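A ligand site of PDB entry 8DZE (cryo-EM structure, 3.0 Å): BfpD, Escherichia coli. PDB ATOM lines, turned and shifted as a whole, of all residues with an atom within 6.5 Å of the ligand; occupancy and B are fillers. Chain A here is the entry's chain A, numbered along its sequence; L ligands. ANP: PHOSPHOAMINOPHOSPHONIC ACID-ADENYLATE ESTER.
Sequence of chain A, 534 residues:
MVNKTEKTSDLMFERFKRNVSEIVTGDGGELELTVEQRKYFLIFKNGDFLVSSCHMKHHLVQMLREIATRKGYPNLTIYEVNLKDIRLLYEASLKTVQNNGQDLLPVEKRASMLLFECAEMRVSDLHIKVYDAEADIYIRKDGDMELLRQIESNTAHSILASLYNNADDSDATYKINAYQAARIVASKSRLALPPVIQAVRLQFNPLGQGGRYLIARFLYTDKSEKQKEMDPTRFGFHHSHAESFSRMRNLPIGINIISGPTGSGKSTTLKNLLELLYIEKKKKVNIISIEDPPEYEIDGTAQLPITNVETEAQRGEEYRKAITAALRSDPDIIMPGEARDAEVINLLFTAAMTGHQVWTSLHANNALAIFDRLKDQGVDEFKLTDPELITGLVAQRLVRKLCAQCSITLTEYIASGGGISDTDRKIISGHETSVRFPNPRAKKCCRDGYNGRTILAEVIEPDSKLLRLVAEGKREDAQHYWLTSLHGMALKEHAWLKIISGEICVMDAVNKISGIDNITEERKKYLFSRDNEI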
ATOM      1  N   SER A 124     -24.213  11.941  -1.382  1.00  0.00           N
ATOM      2  CA  SER A 124     -24.476  12.748  -2.575  1.00  0.00           C
ATOM      3  C   SER A 124     -24.851  14.172  -2.212  1.00  0.00           C
ATOM      4  O   SER A 124     -24.118  15.111  -2.538  1.00  0.00           O
ATOM      5  CB  SER A 124     -25.580  12.088  -3.409  1.00  0.00           C
ATOM      6  OG  SER A 124     -25.179  10.822  -3.886  1.00  0.00           O
ATOM      7  N   ARG A 217     -24.798  20.018  -2.994  1.00  0.00           N
ATOM      8  CA  ARG A 217     -24.800  19.021  -4.065  1.00  0.00           C
ATOM      9  C   ARG A 217     -23.548  18.150  -4.079  1.00  0.00           C
ATOM     10  O   ARG A 217     -23.625  17.005  -4.531  1.00  0.00           O
ATOM     11  CB  ARG A 217     -24.945  19.716  -5.422  1.00  0.00           C
ATOM     12  CG  ARG A 217     -26.386  19.851  -5.896  1.00  0.00           C
ATOM     13  CD  ARG A 217     -27.017  18.481  -6.116  1.00  0.00           C
ATOM     14  NE  ARG A 217     -26.208  17.636  -6.979  1.00  0.00           N
ATOM     15  CZ  ARG A 217     -26.535  16.405  -7.346  1.00  0.00           C
ATOM     16  NH1 ARG A 217     -27.664  15.845  -6.941  1.00  0.00           N
ATOM     17  NH2 ARG A 217     -25.715  15.720  -8.141  1.00  0.00           N
ATOM     18  N   TYR A 220     -18.179  15.821  -7.217  1.00  0.00           N
ATOM     19  CA  TYR A 220     -16.918  15.119  -7.019  1.00  0.00           C
ATOM     20  C   TYR A 220     -16.109  15.123  -8.307  1.00  0.00           C
ATOM     21  O   TYR A 220     -16.660  15.000  -9.409  1.00  0.00           O
ATOM     22  CB  TYR A 220     -17.166  13.679  -6.571  1.00  0.00           C
ATOM     23  CG  TYR A 220     -17.731  13.550  -5.173  1.00  0.00           C
ATOM     24  CD1 TYR A 220     -16.953  13.821  -4.066  1.00  0.00           C
ATOM     25  CD2 TYR A 220     -19.050  13.149  -4.987  1.00  0.00           C
ATOM     26  CE1 TYR A 220     -17.461  13.703  -2.785  1.00  0.00           C
ATOM     27  CE2 TYR A 220     -19.574  13.029  -3.706  1.00  0.00           C
ATOM     28  CZ  TYR A 220     -18.781  13.308  -2.612  1.00  0.00           C
ATOM     29  OH  TYR A 220     -19.295  13.188  -1.348  1.00  0.00           O
ATOM     30  N   PHE A 235     -22.250  -3.159 -16.401  1.00  0.00           N
ATOM     31  CA  PHE A 235     -22.507  -2.634 -15.060  1.00  0.00           C
ATOM     32  C   PHE A 235     -23.779  -3.237 -14.486  1.00  0.00           C
ATOM     33  O   PHE A 235     -23.748  -3.968 -13.480  1.00  0.00           O
ATOM     34  CB  PHE A 235     -22.600  -1.109 -15.097  1.00  0.00           C
ATOM     35  CG  PHE A 235     -21.327  -0.437 -15.502  1.00  0.00           C
ATOM     36  CD1 PHE A 235     -20.139  -0.727 -14.847  1.00  0.00           C
ATOM     37  CD2 PHE A 235     -21.299   0.497 -16.528  1.00  0.00           C
ATOM     38  CE1 PHE A 235     -18.961  -0.103 -15.207  1.00  0.00           C
ATOM     39  CE2 PHE A 235     -20.126   1.112 -16.892  1.00  0.00           C
ATOM     40  CZ  PHE A 235     -18.955   0.819 -16.236  1.00  0.00           C
ATOM     41  N   GLY A 236     -24.918  -2.949 -15.109  1.00  0.00           N
ATOM     42  CA  GLY A 236     -26.180  -3.566 -14.743  1.00  0.00           C
ATOM     43  C   GLY A 236     -27.033  -3.868 -15.948  1.00  0.00           C
ATOM     44  O   GLY A 236     -28.164  -4.349 -15.819  1.00  0.00           O
ATOM     45  N   PRO A 261     -34.022  10.000 -14.319  1.00  0.00           N
ATOM     46  CA  PRO A 261     -34.009  10.966 -13.216  1.00  0.00           C
ATOM     47  C   PRO A 261     -32.602  11.441 -12.854  1.00  0.00           C
ATOM     48  O   PRO A 261     -31.629  11.093 -13.523  1.00  0.00           O
ATOM     49  CB  PRO A 261     -34.662  10.195 -12.060  1.00  0.00           C
ATOM     50  CG  PRO A 261     -34.538   8.755 -12.431  1.00  0.00           C
ATOM     51  CD  PRO A 261     -34.660   8.731 -13.921  1.00  0.00           C
ATOM     52  N   THR A 262     -32.509  12.244 -11.784  1.00  0.00           N
ATOM     53  CA  THR A 262     -31.249  12.887 -11.433  1.00  0.00           C
ATOM     54  C   THR A 262     -30.167  11.867 -11.080  1.00  0.00           C
ATOM     55  O   THR A 262     -29.013  12.002 -11.508  1.00  0.00           O
ATOM     56  CB  THR A 262     -31.479  13.853 -10.262  1.00  0.00           C
ATOM     57  OG1 THR A 262     -32.455  14.833 -10.630  1.00  0.00           O
ATOM     58  CG2 THR A 262     -30.176  14.563  -9.895  1.00  0.00           C
ATOM     59  N   GLY A 263     -30.518  10.841 -10.302  1.00  0.00           N
ATOM     60  CA  GLY A 263     -29.535   9.868  -9.894  1.00  0.00           C
ATOM     61  C   GLY A 263     -29.457   8.658 -10.795  1.00  0.00           C
ATOM     62  O   GLY A 263     -29.299   7.524 -10.319  1.00  0.00           O
ATOM     63  N   SER A 264     -29.548   8.876 -12.108  1.00  0.00           N
ATOM     64  CA  SER A 264     -29.513   7.768 -13.061  1.00  0.00           C
ATOM     65  C   SER A 264     -28.087   7.260 -13.280  1.00  0.00           C
ATOM     66  O   SER A 264     -27.877   6.058 -13.450  1.00  0.00           O
ATOM     67  CB  SER A 264     -30.116   8.198 -14.384  1.00  0.00           C
ATOM     68  OG  SER A 264     -31.523   8.255 -14.300  1.00  0.00           O
ATOM     69  N   GLY A 265     -27.104   8.162 -13.288  1.00  0.00           N
ATOM     70  CA  GLY A 265     -25.743   7.761 -13.608  1.00  0.00           C
ATOM     71  C   GLY A 265     -25.475   7.821 -15.093  1.00  0.00           C
ATOM     72  O   GLY A 265     -24.838   6.935 -15.651  1.00  0.00           O
ATOM     73  N   LYS A 266     -25.957   8.886 -15.746  1.00  0.00           N
ATOM     74  CA  LYS A 266     -25.792   9.012 -17.191  1.00  0.00           C
ATOM     75  C   LYS A 266     -24.361   9.392 -17.555  1.00  0.00           C
ATOM     76  O   LYS A 266     -23.870   8.982 -18.611  1.00  0.00           O
ATOM     77  CB  LYS A 266     -26.769  10.045 -17.737  1.00  0.00           C
ATOM     78  CG  LYS A 266     -28.227   9.754 -17.378  1.00  0.00           C
ATOM     79  CD  LYS A 266     -29.156  10.825 -17.906  1.00  0.00           C
ATOM     80  CE  LYS A 266     -28.987  12.129 -17.141  1.00  0.00           C
ATOM     81  NZ  LYS A 266     -29.422  11.995 -15.729  1.00  0.00           N
ATOM     82  N   SER A 267     -23.695  10.178 -16.707  1.00  0.00           N
ATOM     83  CA  SER A 267     -22.314  10.565 -16.984  1.00  0.00           C
ATOM     84  C   SER A 267     -21.374   9.361 -16.964  1.00  0.00           C
ATOM     85  O   SER A 267     -20.457   9.268 -17.787  1.00  0.00           O
ATOM     86  CB  SER A 267     -21.852  11.621 -15.981  1.00  0.00           C
ATOM     87  OG  SER A 267     -22.653  12.785 -16.066  1.00  0.00           O
ATOM     88  N   THR A 268     -21.593   8.426 -16.040  1.00  0.00           N
ATOM     89  CA  THR A 268     -20.786   7.215 -15.999  1.00  0.00           C
ATOM     90  C   THR A 268     -20.985   6.367 -17.246  1.00  0.00           C
ATOM     91  O   THR A 268     -20.017   5.841 -17.812  1.00  0.00           O
ATOM     92  CB  THR A 268     -21.118   6.411 -14.741  1.00  0.00           C
ATOM     93  OG1 THR A 268     -20.930   7.226 -13.584  1.00  0.00           O
ATOM     94  CG2 THR A 268     -20.228   5.179 -14.634  1.00  0.00           C
ATOM     95  N   THR A 269     -22.234   6.249 -17.705  1.00  0.00           N
ATOM     96  CA  THR A 269     -22.508   5.505 -18.930  1.00  0.00           C
ATOM     97  C   THR A 269     -21.862   6.168 -20.139  1.00  0.00           C
ATOM     98  O   THR A 269     -21.281   5.492 -20.995  1.00  0.00           O
ATOM     99  CB  THR A 269     -24.027   5.381 -19.135  1.00  0.00           C
ATOM    100  OG1 THR A 269     -24.607   4.683 -18.026  1.00  0.00           O
ATOM    101  CG2 THR A 269     -24.338   4.632 -20.419  1.00  0.00           C
ATOM    102  N   GLU A 295     -15.659  16.541 -14.441  1.00  0.00           N
ATOM    103  CA  GLU A 295     -15.932  15.436 -13.529  1.00  0.00           C
ATOM    104  C   GLU A 295     -15.465  14.149 -14.177  1.00  0.00           C
ATOM    105  O   GLU A 295     -15.900  13.822 -15.288  1.00  0.00           O
ATOM    106  CB  GLU A 295     -17.421  15.356 -13.176  1.00  0.00           C
ATOM    107  CG  GLU A 295     -17.815  14.097 -12.416  1.00  0.00           C
ATOM    108  CD  GLU A 295     -18.704  13.181 -13.231  1.00  0.00           C
ATOM    109  OE1 GLU A 295     -19.620  13.690 -13.909  1.00  0.00           O
ATOM    110  OE2 GLU A 295     -18.490  11.946 -13.184  1.00  0.00           O
ATOM    111  N   GLU A 338     -25.053  17.161 -21.246  1.00  0.00           N
ATOM    112  CA  GLU A 338     -26.424  17.495 -20.861  1.00  0.00           C
ATOM    113  C   GLU A 338     -27.066  18.384 -21.942  1.00  0.00           C
ATOM    114  O   GLU A 338     -26.449  18.611 -22.995  1.00  0.00           O
ATOM    115  CB  GLU A 338     -26.393  18.136 -19.450  1.00  0.00           C
ATOM    116  CG  GLU A 338     -27.722  18.475 -18.750  1.00  0.00           C
ATOM    117  CD  GLU A 338     -28.505  17.231 -18.364  1.00  0.00           C
ATOM    118  OE1 GLU A 338     -27.896  16.281 -17.854  1.00  0.00           O
ATOM    119  OE2 GLU A 338     -29.734  17.229 -18.582  1.00  0.00           O
ATOM    120  N   HIS A 363     -33.301  14.636 -19.512  1.00  0.00           N
ATOM    121  CA  HIS A 363     -34.130  14.266 -18.371  1.00  0.00           C
ATOM    122  C   HIS A 363     -35.509  13.858 -18.893  1.00  0.00           C
ATOM    123  O   HIS A 363     -36.302  14.715 -19.297  1.00  0.00           O
ATOM    124  CB  HIS A 363     -34.242  15.423 -17.372  1.00  0.00           C
ATOM    125  CG  HIS A 363     -33.102  15.498 -16.400  1.00  0.00           C
ATOM    126  ND1 HIS A 363     -32.080  16.408 -16.525  1.00  0.00           N
ATOM    127  CD2 HIS A 363     -32.828  14.777 -15.295  1.00  0.00           C
ATOM    128  CE1 HIS A 363     -31.227  16.248 -15.527  1.00  0.00           C
ATOM    129  NE2 HIS A 363     -31.662  15.263 -14.768  1.00  0.00           N
ATOM    130  N   GLN A 396     -32.617   4.888 -18.158  1.00  0.00           N
ATOM    131  CA  GLN A 396     -32.042   4.070 -17.107  1.00  0.00           C
ATOM    132  C   GLN A 396     -32.337   4.650 -15.731  1.00  0.00           C
ATOM    133  O   GLN A 396     -32.541   5.852 -15.569  1.00  0.00           O
ATOM    134  CB  GLN A 396     -30.525   3.928 -17.288  1.00  0.00           C
ATOM    135  CG  GLN A 396     -29.757   5.222 -17.194  1.00  0.00           C
ATOM    136  CD  GLN A 396     -28.280   5.049 -17.461  1.00  0.00           C
ATOM    137  OE1 GLN A 396     -27.811   3.931 -17.688  1.00  0.00           O
ATOM    138  NE2 GLN A 396     -27.536   6.149 -17.456  1.00  0.00           N
ATOM    139  N   LEU A 398     -31.232   3.798 -11.312  1.00  0.00           N
ATOM    140  CA  LEU A 398     -30.311   3.149 -10.392  1.00  0.00           C
ATOM    141  C   LEU A 398     -31.058   2.675  -9.152  1.00  0.00           C
ATOM    142  O   LEU A 398     -31.786   3.458  -8.534  1.00  0.00           O
ATOM    143  CB  LEU A 398     -29.177   4.102  -9.978  1.00  0.00           C
ATOM    144  CG  LEU A 398     -27.880   4.048 -10.791  1.00  0.00           C
ATOM    145  CD1 LEU A 398     -26.961   5.193 -10.385  1.00  0.00           C
ATOM    146  CD2 LEU A 398     -27.191   2.717 -10.602  1.00  0.00           C
ATOM    147  N   GLY A 452     -23.575  -1.530  -3.205  1.00  0.00           N
ATOM    148  CA  GLY A 452     -23.570  -0.713  -4.402  1.00  0.00           C
ATOM    149  C   GLY A 452     -24.952  -0.546  -5.018  1.00  0.00           C
ATOM    150  O   GLY A 452     -25.992  -0.703  -4.373  1.00  0.00           O
ATOM    151  N   ARG A 453     -24.951  -0.208  -6.305  1.00  0.00           N
ATOM    152  CA  ARG A 453     -26.171   0.038  -7.053  1.00  0.00           C
ATOM    153  C   ARG A 453     -26.040  -0.552  -8.453  1.00  0.00           C
ATOM    154  O   ARG A 453     -24.938  -0.753  -8.965  1.00  0.00           O
ATOM    155  CB  ARG A 453     -26.501   1.530  -7.138  1.00  0.00           C
ATOM    156  CG  ARG A 453     -27.346   2.047  -5.978  1.00  0.00           C
ATOM    157  CD  ARG A 453     -27.807   3.469  -6.232  1.00  0.00           C
ATOM    158  NE  ARG A 453     -26.693   4.411  -6.285  1.00  0.00           N
ATOM    159  CZ  ARG A 453     -26.820   5.708  -6.502  1.00  0.00           C
ATOM    160  NH1 ARG A 453     -28.003   6.264  -6.710  1.00  0.00           N
ATOM    161  NH2 ARG A 453     -25.726   6.470  -6.522  1.00  0.00           N
ATOM    162  N   THR A 454     -27.192  -0.836  -9.064  1.00  0.00           N
ATOM    163  CA  THR A 454     -27.260  -1.411 -10.403  1.00  0.00           C
ATOM    164  C   THR A 454     -28.234  -0.606 -11.249  1.00  0.00           C
ATOM    165  O   THR A 454     -29.157   0.051 -10.748  1.00  0.00           O
ATOM    166  CB  THR A 454     -27.699  -2.880 -10.379  1.00  0.00           C
ATOM    167  OG1 THR A 454     -28.942  -3.003  -9.687  1.00  0.00           O
ATOM    168  CG2 THR A 454     -26.653  -3.742  -9.714  1.00  0.00           C
ATOM    169  N   ILE A 455     -28.033  -0.690 -12.564  1.00  0.00           N
ATOM    170  CA  ILE A 455     -28.810   0.056 -13.544  1.00  0.00           C
ATOM    171  C   ILE A 455     -29.863  -0.873 -14.143  1.00  0.00           C
ATOM    172  O   ILE A 455     -29.551  -1.984 -14.581  1.00  0.00           O
ATOM    173  CB  ILE A 455     -27.907   0.654 -14.634  1.00  0.00           C
ATOM    174  CG1 ILE A 455     -27.392   2.031 -14.227  1.00  0.00           C
ATOM    175  CG2 ILE A 455     -28.640   0.778 -15.972  1.00  0.00           C
ATOM    176  CD1 ILE A 455     -26.097   2.413 -14.883  1.00  0.00           C
HETATM  177  PG  ANP L   1     -27.069  14.767 -12.486  1.00  0.00           P
HETATM  178  O1G ANP L   1     -28.318  14.744 -13.338  1.00  0.00           O
HETATM  179  O2G ANP L   1     -25.914  15.303 -13.292  1.00  0.00           O
HETATM  180  O3G ANP L   1     -27.305  15.642 -11.284  1.00  0.00           O
HETATM  181  PB  ANP L   1     -26.057  12.034 -13.040  1.00  0.00           P
HETATM  182  O1B ANP L   1     -27.119  11.577 -14.000  1.00  0.00           O
HETATM  183  O2B ANP L   1     -24.915  12.658 -13.806  1.00  0.00           O
HETATM  184  N3B ANP L   1     -26.719  13.175 -11.959  1.00  0.00           N
HETATM  185  PA  ANP L   1     -23.914  10.442 -11.890  1.00  0.00           P
HETATM  186  O1A ANP L   1     -23.355  11.499 -10.967  1.00  0.00           O
HETATM  187  O2A ANP L   1     -23.141  10.446 -13.189  1.00  0.00           O
HETATM  188  O3A ANP L   1     -25.498  10.745 -12.182  1.00  0.00           O
HETATM  189  O5' ANP L   1     -23.751   8.967 -11.174  1.00  0.00           O
HETATM  190  C5' ANP L   1     -24.514   8.694 -10.038  1.00  0.00           C
HETATM  191  C4' ANP L   1     -23.666   7.876  -9.035  1.00  0.00           C
HETATM  192  O4' ANP L   1     -24.045   6.633  -9.030  1.00  0.00           O
HETATM  193  C3' ANP L   1     -22.196   7.835  -9.485  1.00  0.00           C
HETATM  194  O3' ANP L   1     -21.443   8.669  -8.735  1.00  0.00           O
HETATM  195  C2' ANP L   1     -21.741   6.371  -9.270  1.00  0.00           C
HETATM  196  O2' ANP L   1     -20.497   6.347  -8.446  1.00  0.00           O
HETATM  197  C1' ANP L   1     -22.729   5.804  -8.630  1.00  0.00           C
HETATM  198  N9  ANP L   1     -22.868   4.422  -9.030  1.00  0.00           N
HETATM  199  C8  ANP L   1     -22.728   3.329  -8.278  1.00  0.00           C
HETATM  200  N7  ANP L   1     -22.939   2.269  -9.057  1.00  0.00           N
HETATM  201  C5  ANP L   1     -23.211   2.702 -10.294  1.00  0.00           C
HETATM  202  C6  ANP L   1     -23.490   2.036 -11.462  1.00  0.00           C
HETATM  203  N6  ANP L   1     -23.590   0.607 -11.693  1.00  0.00           N
HETATM  204  N1  ANP L   1     -23.717   2.721 -12.572  1.00  0.00           N
HETATM  205  C2  ANP L   1     -23.667   4.075 -12.553  1.00  0.00           C
HETATM  206  N3  ANP L   1     -23.386   4.724 -11.409  1.00  0.00           N
HETATM  207  C4  ANP L   1     -23.153   4.042 -10.282  1.00  0.00           C
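The backbone carbonyl oxygen (O) of Thr 262 lies within hydrogen-bond range of a nitrogen (N3B) of the ligand (2.6 Å). An oxygen (O1B) of the ligand is in hydrogen-bond range of the backbone NH of Lys 266 (3.4 Å). The side-chain amino group (NZ) of Lys 266 is in salt-bridge range of an oxygen (O1B) of the ligand, at 2.9 Å. O of Arg 453 sits at hydrogen-bond distance from N6 of the ligand (3.3 Å). The guanidinium group of Arg 453 sits at hydrogen-bond distance from an oxygen (O4') of the ligand (3.0 Å). OG of Ser 267 sits at hydrogen-bond distance from O2B of the ligand (3.2 Å). An oxygen (O3A) of the ligand sits at hydrogen-bond distance from the backbone NH of Gly 265 (3.2 Å). NH2 of Arg 217 is in salt-bridge range of O3G of the ligand.
NZ of Lys 266 sits at hydrogen-bond distance from O of Pro 261. OG1 of Thr 269 lies within hydrogen-bond range of O of Gly 265, 3.3 Å away. O of Gly 265 is in hydrogen-bond range of NE2 of Gln 396 (3.3 Å). ND1 of His 363 is in hydrogen-bond range of OE2 of Glu 338 (3.2 Å).
Phe 235 touches the ligand. Thr 268 touches the ligand (N to O2A, 3.8 Å). NE2 of His 363 touches O1G of the ligand (3.7 Å). CD1 of Leu 398 touches O4' of the ligand, 3.5 Å away. CD1 of Ile 455 touches N1 of the ligand, at 3.3 Å. Hydrophobic or aromatic side chains that line the ligand: Phe 235, His 363, Leu 398 and Ile 455. 11 residues have an atom within 4 Å of the ligand: Arg 217, Phe 235, Thr 262, Gly 265, Lys 266, Ser 267, Thr 268, His 363, Leu 398, Arg 453 and Ile 455.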
